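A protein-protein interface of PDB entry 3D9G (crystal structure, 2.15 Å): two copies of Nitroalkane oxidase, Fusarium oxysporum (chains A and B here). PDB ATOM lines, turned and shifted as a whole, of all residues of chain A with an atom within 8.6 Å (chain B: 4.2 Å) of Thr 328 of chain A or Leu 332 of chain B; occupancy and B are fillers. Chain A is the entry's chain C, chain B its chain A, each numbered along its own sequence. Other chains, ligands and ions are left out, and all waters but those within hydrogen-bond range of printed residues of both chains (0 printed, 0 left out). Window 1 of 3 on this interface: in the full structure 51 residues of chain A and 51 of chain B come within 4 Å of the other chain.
Of chain B, only Leu 332 comes within 4 Å of Thr 328 of chain A. Of chain A, only Glu 327, Thr 328 and Leu 331 come within 4 Å of Leu 332 of chain B. Of the printed residues of chain A, Trp 334 of chain B touches Phe 3. Printed residues of chain B within 4 Å of Lys 323 of chain A: Gln 356. Printed residues of chain B within 4 Å of Ile 324 of chain A: Gln 356 (3.9 Å) and Tyr 360 (3.5 Å). Val 333 of chain A touches none of the printed residues of chain B. The nearest residue of chain B that does not touch Thr 328 of chain A is Tyr 360 of chain B (4.1 Å).
The side-chain hydroxyl of Thr 328 of chain B sits at hydrogen-bond distance from the side-chain hydroxyl of Tyr 360 of chain B, 2.6 Å away. The side-chain hydroxyl (OG1) of Thr 328 of chain A is in hydrogen-bond range of the backbone carbonyl oxygen (O) of Ile 324 of chain A (2.8 Å). The side-chain hydroxyl (OG1) of Thr 328 of chain A sits at hydrogen-bond distance from the backbone carbonyl oxygen (O) of Arg 325 of chain A. NH1 of Arg 330 of chain A is in salt-bridge range of OE1 of Glu 327 of chain A. The side-chain hydroxyl of Thr 328 of chain A is in hydrogen-bond range of the side-chain hydroxyl of Tyr 360 of chain A, at 2.7 Å.
Thr 328 of chain A touches Leu 332 of chain B, and with the chains exchanged Leu 332 of chain A touches Thr 328 of chain B. Leu 331 of chain A touches its own counterpart, Leu 331 of chain B. Leu 331 of chain A touches Lys 335 of chain B, and with the chains exchanged Lys 335 of chain A touches Leu 331 of chain B. Tyr 360 of chain A touches its own counterpart, Tyr 360 of chain B. Positions printed for both chains: 328, 329, 330, 331, 332, 333, 334, 335, 357 and 360. Of the 15 pairs that touch across the chains among the printed residues, 8 have their exchanged pair printed and touching as well.
OE1 of Gln 356 of chain B is in hydrogen-bond range of NZ of Lys 323 of chain A (3.4 Å).
Phe 3 of chain A touches Trp 334 of chain B (CE1 to O, 3.7 Å). Phe 3 of chain A touches Lys 335 of chain B (CE1 to CA, 3.6 Å). O of Gln 356 of chain B touches CD1 of Ile 324 of chain A (3.9 Å). CG2 of Ile 324 of chain A touches CD1 of Tyr 360 of chain B, 3.5 Å away. CG of Glu 327 of chain A touches CD1 of Leu 332 of chain B, at 3.9 Å. Glu 327 of chain A touches Gln 356 of chain B (CB to NE2, 3.3 Å). CD2 of Leu 331 of chain A touches CA of Leu 332 of chain B (3.7 Å). Leu 331 of chain A touches Lys 335 of chain B. Thr 328 of chain B touches Leu 332 of chain A (CG2 to CD2, 3.8 Å). OH of Tyr 360 of chain A touches OH of Tyr 360 of chain B (3.7 Å).
Hydrophobic or aromatic side chains of chain B within 4 Å of the printed part of chain A: Leu 331, Leu 332 and Tyr 360. Printed residues of chain A that touch a printed residue of chain B: Phe 3, Lys 323, Ile 324, Glu 327, Thr 328, Leu 331, Leu 332, Lys 335 and Tyr 360. Hydrophobic or aromatic side chains of chain A within 4 Å of the printed part of chain B: Phe 3, Ile 324, Leu 331, Leu 332 and Tyr 360. Among the printed residues, 15 pairs touch across the chains.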
ATOM      1  N   PHE A   3      21.841 -14.396   6.361  1.00  0.00           N
ATOM      2  CA  PHE A   3      20.849 -15.467   6.206  1.00  0.00           C
ATOM      3  C   PHE A   3      19.476 -15.092   6.731  1.00  0.00           C
ATOM      4  O   PHE A   3      18.567 -15.924   6.725  1.00  0.00           O
ATOM      5  CB  PHE A   3      21.310 -16.750   6.909  1.00  0.00           C
ATOM      6  CG  PHE A   3      22.485 -17.405   6.261  1.00  0.00           C
ATOM      7  CD1 PHE A   3      23.771 -17.154   6.719  1.00  0.00           C
ATOM      8  CD2 PHE A   3      22.307 -18.274   5.192  1.00  0.00           C
ATOM      9  CE1 PHE A   3      24.868 -17.757   6.116  1.00  0.00           C
ATOM     10  CE2 PHE A   3      23.397 -18.886   4.586  1.00  0.00           C
ATOM     11  CZ  PHE A   3      24.677 -18.632   5.049  1.00  0.00           C
ATOM     12  N   ILE A 284      13.327 -31.189  -0.043  1.00  0.00           N
ATOM     13  CA  ILE A 284      13.386 -30.759   1.354  1.00  0.00           C
ATOM     14  C   ILE A 284      12.021 -30.887   2.037  1.00  0.00           C
ATOM     15  O   ILE A 284      11.935 -31.429   3.137  1.00  0.00           O
ATOM     16  CB  ILE A 284      13.948 -29.332   1.515  1.00  0.00           C
ATOM     17  CG1 ILE A 284      15.435 -29.308   1.180  1.00  0.00           C
ATOM     18  CG2 ILE A 284      13.748 -28.824   2.940  1.00  0.00           C
ATOM     19  CD1 ILE A 284      15.982 -27.879   0.897  1.00  0.00           C
ATOM     20  N   ASP A 321      21.378 -37.348  11.442  1.00  0.00           N
ATOM     21  CA  ASP A 321      21.721 -37.445  10.025  1.00  0.00           C
ATOM     22  C   ASP A 321      20.631 -36.830   9.140  1.00  0.00           C
ATOM     23  O   ASP A 321      20.941 -36.137   8.176  1.00  0.00           O
ATOM     24  CB  ASP A 321      21.986 -38.894   9.630  1.00  0.00           C
ATOM     25  CG  ASP A 321      23.212 -39.471  10.317  1.00  0.00           C
ATOM     26  OD1 ASP A 321      23.361 -40.708  10.300  1.00  0.00           O
ATOM     27  OD2 ASP A 321      24.025 -38.698  10.864  1.00  0.00           O
ATOM     28  N   CYS A 322      19.366 -37.082   9.483  1.00  0.00           N
ATOM     29  CA  CYS A 322      18.238 -36.411   8.837  1.00  0.00           C
ATOM     30  C   CYS A 322      18.346 -34.877   8.915  1.00  0.00           C
ATOM     31  O   CYS A 322      18.264 -34.193   7.893  1.00  0.00           O
ATOM     32  CB  CYS A 322      16.923 -36.849   9.474  1.00  0.00           C
ATOM     33  SG  CYS A 322      16.467 -38.568   9.142  1.00  0.00           S
ATOM     34  N   LYS A 323      18.491 -34.344  10.122  1.00  0.00           N
ATOM     35  CA  LYS A 323      18.505 -32.897  10.334  1.00  0.00           C
ATOM     36  C   LYS A 323      19.643 -32.266   9.517  1.00  0.00           C
ATOM     37  O   LYS A 323      19.439 -31.284   8.826  1.00  0.00           O
ATOM     38  CB  LYS A 323      18.674 -32.579  11.833  1.00  0.00           C
ATOM     39  CG  LYS A 323      18.759 -31.068  12.212  1.00  0.00           C
ATOM     40  CD  LYS A 323      17.475 -30.334  11.828  1.00  0.00           C
ATOM     41  CE  LYS A 323      17.118 -29.151  12.747  1.00  0.00           C
ATOM     42  NZ  LYS A 323      18.204 -28.178  13.000  1.00  0.00           N
ATOM     43  N   ILE A 324      20.832 -32.859   9.594  1.00  0.00           N
ATOM     44  CA  ILE A 324      22.001 -32.401   8.844  1.00  0.00           C
ATOM     45  C   ILE A 324      21.772 -32.347   7.322  1.00  0.00           C
ATOM     46  O   ILE A 324      22.147 -31.365   6.646  1.00  0.00           O
ATOM     47  CB  ILE A 324      23.250 -33.269   9.201  1.00  0.00           C
ATOM     48  CG1 ILE A 324      23.745 -32.922  10.612  1.00  0.00           C
ATOM     49  CG2 ILE A 324      24.325 -33.091   8.163  1.00  0.00           C
ATOM     50  CD1 ILE A 324      24.894 -33.772  11.168  1.00  0.00           C
ATOM     51  N   ARG A 325      21.176 -33.407   6.783  1.00  0.00           N
ATOM     52  CA  ARG A 325      20.823 -33.461   5.368  1.00  0.00           C
ATOM     53  C   ARG A 325      19.845 -32.358   4.981  1.00  0.00           C
ATOM     54  O   ARG A 325      19.962 -31.775   3.915  1.00  0.00           O
ATOM     55  CB  ARG A 325      20.224 -34.831   5.018  1.00  0.00           C
ATOM     56  CG  ARG A 325      21.262 -35.932   5.017  1.00  0.00           C
ATOM     57  CD  ARG A 325      20.671 -37.288   4.704  1.00  0.00           C
ATOM     58  NE  ARG A 325      21.774 -38.228   4.522  1.00  0.00           N
ATOM     59  CZ  ARG A 325      22.000 -39.285   5.291  1.00  0.00           C
ATOM     60  NH1 ARG A 325      23.054 -40.058   5.049  1.00  0.00           N
ATOM     61  NH2 ARG A 325      21.173 -39.586   6.277  1.00  0.00           N
ATOM     62  N   LEU A 326      18.872 -32.090   5.844  1.00  0.00           N
ATOM     63  CA  LEU A 326      17.853 -31.090   5.552  1.00  0.00           C
ATOM     64  C   LEU A 326      18.451 -29.695   5.613  1.00  0.00           C
ATOM     65  O   LEU A 326      18.155 -28.845   4.780  1.00  0.00           O
ATOM     66  CB  LEU A 326      16.687 -31.214   6.522  1.00  0.00           C
ATOM     67  CG  LEU A 326      15.700 -32.352   6.244  1.00  0.00           C
ATOM     68  CD1 LEU A 326      14.915 -32.653   7.495  1.00  0.00           C
ATOM     69  CD2 LEU A 326      14.779 -32.025   5.080  1.00  0.00           C
ATOM     70  N   GLU A 327      19.329 -29.478   6.584  1.00  0.00           N
ATOM     71  CA  GLU A 327      19.921 -28.158   6.804  1.00  0.00           C
ATOM     72  C   GLU A 327      20.877 -27.770   5.662  1.00  0.00           C
ATOM     73  O   GLU A 327      20.786 -26.677   5.108  1.00  0.00           O
ATOM     74  CB  GLU A 327      20.632 -28.119   8.164  1.00  0.00           C
ATOM     75  CG  GLU A 327      21.139 -26.743   8.584  1.00  0.00           C
ATOM     76  CD  GLU A 327      20.033 -25.692   8.641  1.00  0.00           C
ATOM     77  OE1 GLU A 327      19.011 -25.915   9.337  1.00  0.00           O
ATOM     78  OE2 GLU A 327      20.191 -24.649   7.963  1.00  0.00           O
ATOM     79  N   THR A 328      21.774 -28.679   5.312  1.00  0.00           N
ATOM     80  CA  THR A 328      22.686 -28.495   4.196  1.00  0.00           C
ATOM     81  C   THR A 328      21.956 -28.401   2.856  1.00  0.00           C
ATOM     82  O   THR A 328      22.329 -27.586   2.012  1.00  0.00           O
ATOM     83  CB  THR A 328      23.745 -29.627   4.137  1.00  0.00           C
ATOM     84  OG1 THR A 328      23.085 -30.895   4.051  1.00  0.00           O
ATOM     85  CG2 THR A 328      24.612 -29.606   5.387  1.00  0.00           C
ATOM     86  N   SER A 329      20.933 -29.235   2.656  1.00  0.00           N
ATOM     87  CA  SER A 329      20.092 -29.115   1.467  1.00  0.00           C
ATOM     88  C   SER A 329      19.504 -27.694   1.285  1.00  0.00           C
ATOM     89  O   SER A 329      19.582 -27.139   0.196  1.00  0.00           O
ATOM     90  CB  SER A 329      18.952 -30.140   1.468  1.00  0.00           C
ATOM     91  OG  SER A 329      19.434 -31.429   1.137  1.00  0.00           O
ATOM     92  N   ARG A 330      18.930 -27.125   2.351  1.00  0.00           N
ATOM     93  CA  ARG A 330      18.251 -25.809   2.265  1.00  0.00           C
ATOM     94  C   ARG A 330      19.239 -24.690   1.991  1.00  0.00           C
ATOM     95  O   ARG A 330      18.983 -23.813   1.175  1.00  0.00           O
ATOM     96  CB  ARG A 330      17.429 -25.489   3.524  1.00  0.00           C
ATOM     97  CG  ARG A 330      16.511 -24.257   3.348  1.00  0.00           C
ATOM     98  CD  ARG A 330      15.771 -23.849   4.635  1.00  0.00           C
ATOM     99  NE  ARG A 330      14.873 -24.897   5.133  1.00  0.00           N
ATOM    100  CZ  ARG A 330      15.103 -25.626   6.227  1.00  0.00           C
ATOM    101  NH1 ARG A 330      16.198 -25.410   6.947  1.00  0.00           N
ATOM    102  NH2 ARG A 330      14.229 -26.556   6.604  1.00  0.00           N
ATOM    103  N   LEU A 331      20.368 -24.720   2.685  1.00  0.00           N
ATOM    104  CA  LEU A 331      21.458 -23.786   2.418  1.00  0.00           C
ATOM    105  C   LEU A 331      21.899 -23.826   0.942  1.00  0.00           C
ATOM    106  O   LEU A 331      22.170 -22.786   0.335  1.00  0.00           O
ATOM    107  CB  LEU A 331      22.633 -24.113   3.320  1.00  0.00           C
ATOM    108  CG  LEU A 331      22.805 -23.387   4.663  1.00  0.00           C
ATOM    109  CD1 LEU A 331      21.537 -22.773   5.193  1.00  0.00           C
ATOM    110  CD2 LEU A 331      23.466 -24.278   5.712  1.00  0.00           C
ATOM    111  N   LEU A 332      21.961 -25.029   0.372  1.00  0.00           N
ATOM    112  CA  LEU A 332      22.457 -25.207  -0.993  1.00  0.00           C
ATOM    113  C   LEU A 332      21.464 -24.656  -1.992  1.00  0.00           C
ATOM    114  O   LEU A 332      21.854 -23.977  -2.942  1.00  0.00           O
ATOM    115  CB  LEU A 332      22.772 -26.682  -1.286  1.00  0.00           C
ATOM    116  CG  LEU A 332      23.512 -27.050  -2.572  1.00  0.00           C
ATOM    117  CD1 LEU A 332      24.881 -26.357  -2.704  1.00  0.00           C
ATOM    118  CD2 LEU A 332      23.690 -28.583  -2.639  1.00  0.00           C
ATOM    119  N   VAL A 333      20.183 -24.924  -1.758  1.00  0.00           N
ATOM    120  CA  VAL A 333      19.107 -24.389  -2.593  1.00  0.00           C
ATOM    121  C   VAL A 333      19.087 -22.856  -2.613  1.00  0.00           C
ATOM    122  O   VAL A 333      18.971 -22.245  -3.680  1.00  0.00           O
ATOM    123  CB  VAL A 333      17.729 -24.927  -2.138  1.00  0.00           C
ATOM    124  CG1 VAL A 333      16.584 -24.199  -2.852  1.00  0.00           C
ATOM    125  CG2 VAL A 333      17.641 -26.435  -2.396  1.00  0.00           C
ATOM    126  N   TRP A 334      19.172 -22.243  -1.433  1.00  0.00           N
ATOM    127  CA  TRP A 334      19.213 -20.783  -1.335  1.00  0.00           C
ATOM    128  C   TRP A 334      20.468 -20.232  -2.017  1.00  0.00           C
ATOM    129  O   TRP A 334      20.389 -19.315  -2.816  1.00  0.00           O
ATOM    130  CB  TRP A 334      19.129 -20.324   0.120  1.00  0.00           C
ATOM    131  CG  TRP A 334      17.787 -20.575   0.762  1.00  0.00           C
ATOM    132  CD1 TRP A 334      16.749 -21.329   0.267  1.00  0.00           C
ATOM    133  CD2 TRP A 334      17.358 -20.093   2.037  1.00  0.00           C
ATOM    134  NE1 TRP A 334      15.701 -21.330   1.155  1.00  0.00           N
ATOM    135  CE2 TRP A 334      16.051 -20.581   2.251  1.00  0.00           C
ATOM    136  CE3 TRP A 334      17.953 -19.287   3.023  1.00  0.00           C
ATOM    137  CZ2 TRP A 334      15.324 -20.289   3.413  1.00  0.00           C
ATOM    138  CZ3 TRP A 334      17.230 -18.995   4.178  1.00  0.00           C
ATOM    139  CH2 TRP A 334      15.929 -19.491   4.359  1.00  0.00           C
ATOM    140  N   LYS A 335      21.623 -20.812  -1.723  1.00  0.00           N
ATOM    141  CA  LYS A 335      22.833 -20.491  -2.469  1.00  0.00           C
ATOM    142  C   LYS A 335      22.617 -20.571  -3.999  1.00  0.00           C
ATOM    143  O   LYS A 335      23.055 -19.672  -4.737  1.00  0.00           O
ATOM    144  CB  LYS A 335      23.996 -21.395  -2.039  1.00  0.00           C
ATOM    145  CG  LYS A 335      25.303 -21.185  -2.827  1.00  0.00           C
ATOM    146  CD  LYS A 335      25.767 -19.714  -2.756  1.00  0.00           C
ATOM    147  CE  LYS A 335      27.167 -19.528  -3.324  1.00  0.00           C
ATOM    148  NZ  LYS A 335      27.631 -18.125  -3.075  1.00  0.00           N
ATOM    149  N   THR A 357      23.134 -28.729  -6.756  1.00  0.00           N
ATOM    150  CA  THR A 357      21.957 -28.604  -5.918  1.00  0.00           C
ATOM    151  C   THR A 357      20.992 -29.732  -6.209  1.00  0.00           C
ATOM    152  O   THR A 357      20.543 -30.416  -5.292  1.00  0.00           O
ATOM    153  CB  THR A 357      21.331 -27.239  -6.126  1.00  0.00           C
ATOM    154  OG1 THR A 357      22.309 -26.262  -5.745  1.00  0.00           O
ATOM    155  CG2 THR A 357      20.073 -27.058  -5.289  1.00  0.00           C
ATOM    156  N   TYR A 360      22.526 -33.241  -5.083  1.00  0.00           N
ATOM    157  CA  TYR A 360      22.679 -33.430  -3.650  1.00  0.00           C
ATOM    158  C   TYR A 360      21.345 -33.574  -2.965  1.00  0.00           C
ATOM    159  O   TYR A 360      21.091 -34.563  -2.262  1.00  0.00           O
ATOM    160  CB  TYR A 360      23.453 -32.263  -3.005  1.00  0.00           C
ATOM    161  CG  TYR A 360      23.592 -32.437  -1.500  1.00  0.00           C
ATOM    162  CD1 TYR A 360      24.491 -33.371  -0.963  1.00  0.00           C
ATOM    163  CD2 TYR A 360      22.790 -31.713  -0.615  1.00  0.00           C
ATOM    164  CE1 TYR A 360      24.620 -33.549   0.411  1.00  0.00           C
ATOM    165  CE2 TYR A 360      22.915 -31.884   0.771  1.00  0.00           C
ATOM    166  CZ  TYR A 360      23.826 -32.808   1.273  1.00  0.00           C
ATOM    167  OH  TYR A 360      23.939 -32.987   2.642  1.00  0.00           O
ATOM    168  N   THR A 361      20.485 -32.579  -3.162  1.00  0.00           N
ATOM    169  CA  THR A 361      19.259 -32.485  -2.372  1.00  0.00           C
ATOM    170  C   THR A 361      18.345 -33.668  -2.665  1.00  0.00           C
ATOM    171  O   THR A 361      17.661 -34.155  -1.790  1.00  0.00           O
ATOM    172  CB  THR A 361      18.482 -31.199  -2.692  1.00  0.00           C
ATOM    173  OG1 THR A 361      18.138 -31.208  -4.087  1.00  0.00           O
ATOM    174  CG2 THR A 361      19.325 -29.929  -2.349  1.00  0.00           C
ATOM    175  N   VAL A 364      19.935 -37.097  -1.077  1.00  0.00           N
ATOM    176  CA  VAL A 364      19.897 -37.169   0.388  1.00  0.00           C
ATOM    177  C   VAL A 364      18.495 -37.082   0.967  1.00  0.00           C
ATOM    178  O   VAL A 364      18.287 -37.455   2.127  1.00  0.00           O
ATOM    179  CB  VAL A 364      20.856 -36.190   1.103  1.00  0.00           C
ATOM    180  CG1 VAL A 364      22.283 -36.318   0.526  1.00  0.00           C
ATOM    181  CG2 VAL A 364      20.338 -34.748   1.075  1.00  0.00           C
ATOM    182  N   THR B 328      28.531 -27.666   0.190  1.00  0.00           N
ATOM    183  CA  THR B 328      27.605 -27.820   1.318  1.00  0.00           C
ATOM    184  C   THR B 328      28.289 -27.514   2.641  1.00  0.00           C
ATOM    185  O   THR B 328      27.701 -26.853   3.489  1.00  0.00           O
ATOM    186  CB  THR B 328      26.947 -29.230   1.364  1.00  0.00           C
ATOM    187  OG1 THR B 328      27.973 -30.232   1.361  1.00  0.00           O
ATOM    188  CG2 THR B 328      26.072 -29.427   0.155  1.00  0.00           C
ATOM    189  N   SER B 329      29.535 -27.963   2.795  1.00  0.00           N
ATOM    190  CA  SER B 329      30.298 -27.714   4.018  1.00  0.00           C
ATOM    191  C   SER B 329      30.512 -26.221   4.331  1.00  0.00           C
ATOM    192  O   SER B 329      30.334 -25.821   5.476  1.00  0.00           O
ATOM    193  CB  SER B 329      31.649 -28.439   3.993  1.00  0.00           C
ATOM    194  OG  SER B 329      31.497 -29.836   4.169  1.00  0.00           O
ATOM    195  N   ARG B 330      30.902 -25.421   3.328  1.00  0.00           N
ATOM    196  CA  ARG B 330      31.170 -23.978   3.532  1.00  0.00           C
ATOM    197  C   ARG B 330      29.902 -23.215   3.822  1.00  0.00           C
ATOM    198  O   ARG B 330      29.890 -22.338   4.667  1.00  0.00           O
ATOM    199  CB  ARG B 330      31.897 -23.343   2.330  1.00  0.00           C
ATOM    200  CG  ARG B 330      32.654 -22.026   2.639  1.00  0.00           C
ATOM    201  CD  ARG B 330      33.685 -21.690   1.557  1.00  0.00           C
ATOM    202  NE  ARG B 330      33.139 -22.134   0.297  1.00  0.00           N
ATOM    203  CZ  ARG B 330      33.734 -22.916  -0.590  1.00  0.00           C
ATOM    204  NH1 ARG B 330      34.994 -23.311  -0.459  1.00  0.00           N
ATOM    205  NH2 ARG B 330      33.037 -23.256  -1.641  1.00  0.00           N
ATOM    206  N   LEU B 331      28.833 -23.545   3.108  1.00  0.00           N
ATOM    207  CA  LEU B 331      27.507 -22.990   3.398  1.00  0.00           C
ATOM    208  C   LEU B 331      27.149 -23.187   4.871  1.00  0.00           C
ATOM    209  O   LEU B 331      26.698 -22.246   5.547  1.00  0.00           O
ATOM    210  CB  LEU B 331      26.451 -23.643   2.495  1.00  0.00           C
ATOM    211  CG  LEU B 331      26.036 -22.975   1.170  1.00  0.00           C
ATOM    212  CD1 LEU B 331      26.939 -21.836   0.778  1.00  0.00           C
ATOM    213  CD2 LEU B 331      25.897 -23.955   0.029  1.00  0.00           C
ATOM    214  N   LEU B 332      27.356 -24.406   5.366  1.00  0.00           N
ATOM    215  CA  LEU B 332      27.031 -24.760   6.750  1.00  0.00           C
ATOM    216  C   LEU B 332      27.902 -24.021   7.783  1.00  0.00           C
ATOM    217  O   LEU B 332      27.407 -23.584   8.807  1.00  0.00           O
ATOM    218  CB  LEU B 332      27.135 -26.285   6.950  1.00  0.00           C
ATOM    219  CG  LEU B 332      26.529 -26.908   8.206  1.00  0.00           C
ATOM    220  CD1 LEU B 332      25.060 -26.572   8.291  1.00  0.00           C
ATOM    221  CD2 LEU B 332      26.706 -28.439   8.221  1.00  0.00           C
ATOM    222  N   VAL B 333      29.192 -23.898   7.506  1.00  0.00           N
ATOM    223  CA  VAL B 333      30.096 -23.133   8.363  1.00  0.00           C
ATOM    224  C   VAL B 333      29.639 -21.668   8.472  1.00  0.00           C
ATOM    225  O   VAL B 333      29.485 -21.139   9.580  1.00  0.00           O
ATOM    226  CB  VAL B 333      31.553 -23.227   7.856  1.00  0.00           C
ATOM    227  CG1 VAL B 333      32.457 -22.183   8.543  1.00  0.00           C
ATOM    228  CG2 VAL B 333      32.094 -24.641   8.073  1.00  0.00           C
ATOM    229  N   TRP B 334      29.382 -21.035   7.325  1.00  0.00           N
ATOM    230  CA  TRP B 334      29.002 -19.618   7.289  1.00  0.00           C
ATOM    231  C   TRP B 334      27.641 -19.419   7.944  1.00  0.00           C
ATOM    232  O   TRP B 334      27.430 -18.426   8.648  1.00  0.00           O
ATOM    233  CB  TRP B 334      29.070 -19.064   5.855  1.00  0.00           C
ATOM    234  CG  TRP B 334      30.487 -18.997   5.297  1.00  0.00           C
ATOM    235  CD1 TRP B 334      31.616 -19.514   5.864  1.00  0.00           C
ATOM    236  CD2 TRP B 334      30.904 -18.407   4.051  1.00  0.00           C
ATOM    237  NE1 TRP B 334      32.713 -19.280   5.054  1.00  0.00           N
ATOM    238  CE2 TRP B 334      32.301 -18.597   3.940  1.00  0.00           C
ATOM    239  CE3 TRP B 334      30.233 -17.732   3.020  1.00  0.00           C
ATOM    240  CZ2 TRP B 334      33.046 -18.122   2.842  1.00  0.00           C
ATOM    241  CZ3 TRP B 334      30.979 -17.270   1.923  1.00  0.00           C
ATOM    242  CH2 TRP B 334      32.364 -17.468   1.848  1.00  0.00           C
ATOM    243  N   LYS B 335      26.739 -20.387   7.769  1.00  0.00           N
ATOM    244  CA  LYS B 335      25.462 -20.372   8.483  1.00  0.00           C
ATOM    245  C   LYS B 335      25.636 -20.481  10.007  1.00  0.00           C
ATOM    246  O   LYS B 335      24.977 -19.757  10.777  1.00  0.00           O
ATOM    247  CB  LYS B 335      24.541 -21.481   7.972  1.00  0.00           C
ATOM    248  CG  LYS B 335      23.285 -21.681   8.789  1.00  0.00           C
ATOM    249  CD  LYS B 335      22.424 -20.432   8.773  1.00  0.00           C
ATOM    250  CE  LYS B 335      21.063 -20.709   9.366  1.00  0.00           C
ATOM    251  NZ  LYS B 335      20.237 -19.499   9.182  1.00  0.00           N
ATOM    252  N   ALA B 336      26.515 -21.389  10.434  1.00  0.00           N
ATOM    253  CA  ALA B 336      26.762 -21.618  11.858  1.00  0.00           C
ATOM    254  C   ALA B 336      27.413 -20.422  12.550  1.00  0.00           C
ATOM    255  O   ALA B 336      26.997 -20.055  13.649  1.00  0.00           O
ATOM    256  CB  ALA B 336      27.595 -22.861  12.060  1.00  0.00           C
ATOM    257  N   GLN B 356      25.979 -29.648  14.465  1.00  0.00           N
ATOM    258  CA  GLN B 356      25.744 -30.121  13.093  1.00  0.00           C
ATOM    259  C   GLN B 356      26.926 -29.877  12.181  1.00  0.00           C
ATOM    260  O   GLN B 356      27.314 -30.742  11.384  1.00  0.00           O
ATOM    261  CB  GLN B 356      24.585 -29.350  12.466  1.00  0.00           C
ATOM    262  CG  GLN B 356      23.245 -29.780  12.898  1.00  0.00           C
ATOM    263  CD  GLN B 356      22.179 -28.919  12.286  1.00  0.00           C
ATOM    264  OE1 GLN B 356      21.644 -28.038  12.938  1.00  0.00           O
ATOM    265  NE2 GLN B 356      21.878 -29.155  11.022  1.00  0.00           N
ATOM    266  N   THR B 357      27.461 -28.663  12.285  1.00  0.00           N
ATOM    267  CA  THR B 357      28.532 -28.199  11.430  1.00  0.00           C
ATOM    268  C   THR B 357      29.788 -29.005  11.696  1.00  0.00           C
ATOM    269  O   THR B 357      30.427 -29.492  10.766  1.00  0.00           O
ATOM    270  CB  THR B 357      28.750 -26.660  11.635  1.00  0.00           C
ATOM    271  OG1 THR B 357      27.487 -25.992  11.447  1.00  0.00           O
ATOM    272  CG2 THR B 357      29.770 -26.103  10.660  1.00  0.00           C
ATOM    273  N   TYR B 360      29.111 -32.786  10.406  1.00  0.00           N
ATOM    274  CA  TYR B 360      29.029 -32.887   8.955  1.00  0.00           C
ATOM    275  C   TYR B 360      30.363 -32.588   8.291  1.00  0.00           C
ATOM    276  O   TYR B 360      30.899 -33.438   7.570  1.00  0.00           O
ATOM    277  CB  TYR B 360      27.904 -32.001   8.364  1.00  0.00           C
ATOM    278  CG  TYR B 360      27.804 -32.117   6.838  1.00  0.00           C
ATOM    279  CD1 TYR B 360      27.205 -33.233   6.238  1.00  0.00           C
ATOM    280  CD2 TYR B 360      28.319 -31.121   6.007  1.00  0.00           C
ATOM    281  CE1 TYR B 360      27.122 -33.356   4.857  1.00  0.00           C
ATOM    282  CE2 TYR B 360      28.243 -31.236   4.605  1.00  0.00           C
ATOM    283  CZ  TYR B 360      27.647 -32.363   4.045  1.00  0.00           C
ATOM    284  OH  TYR B 360      27.570 -32.487   2.676  1.00  0.00           O
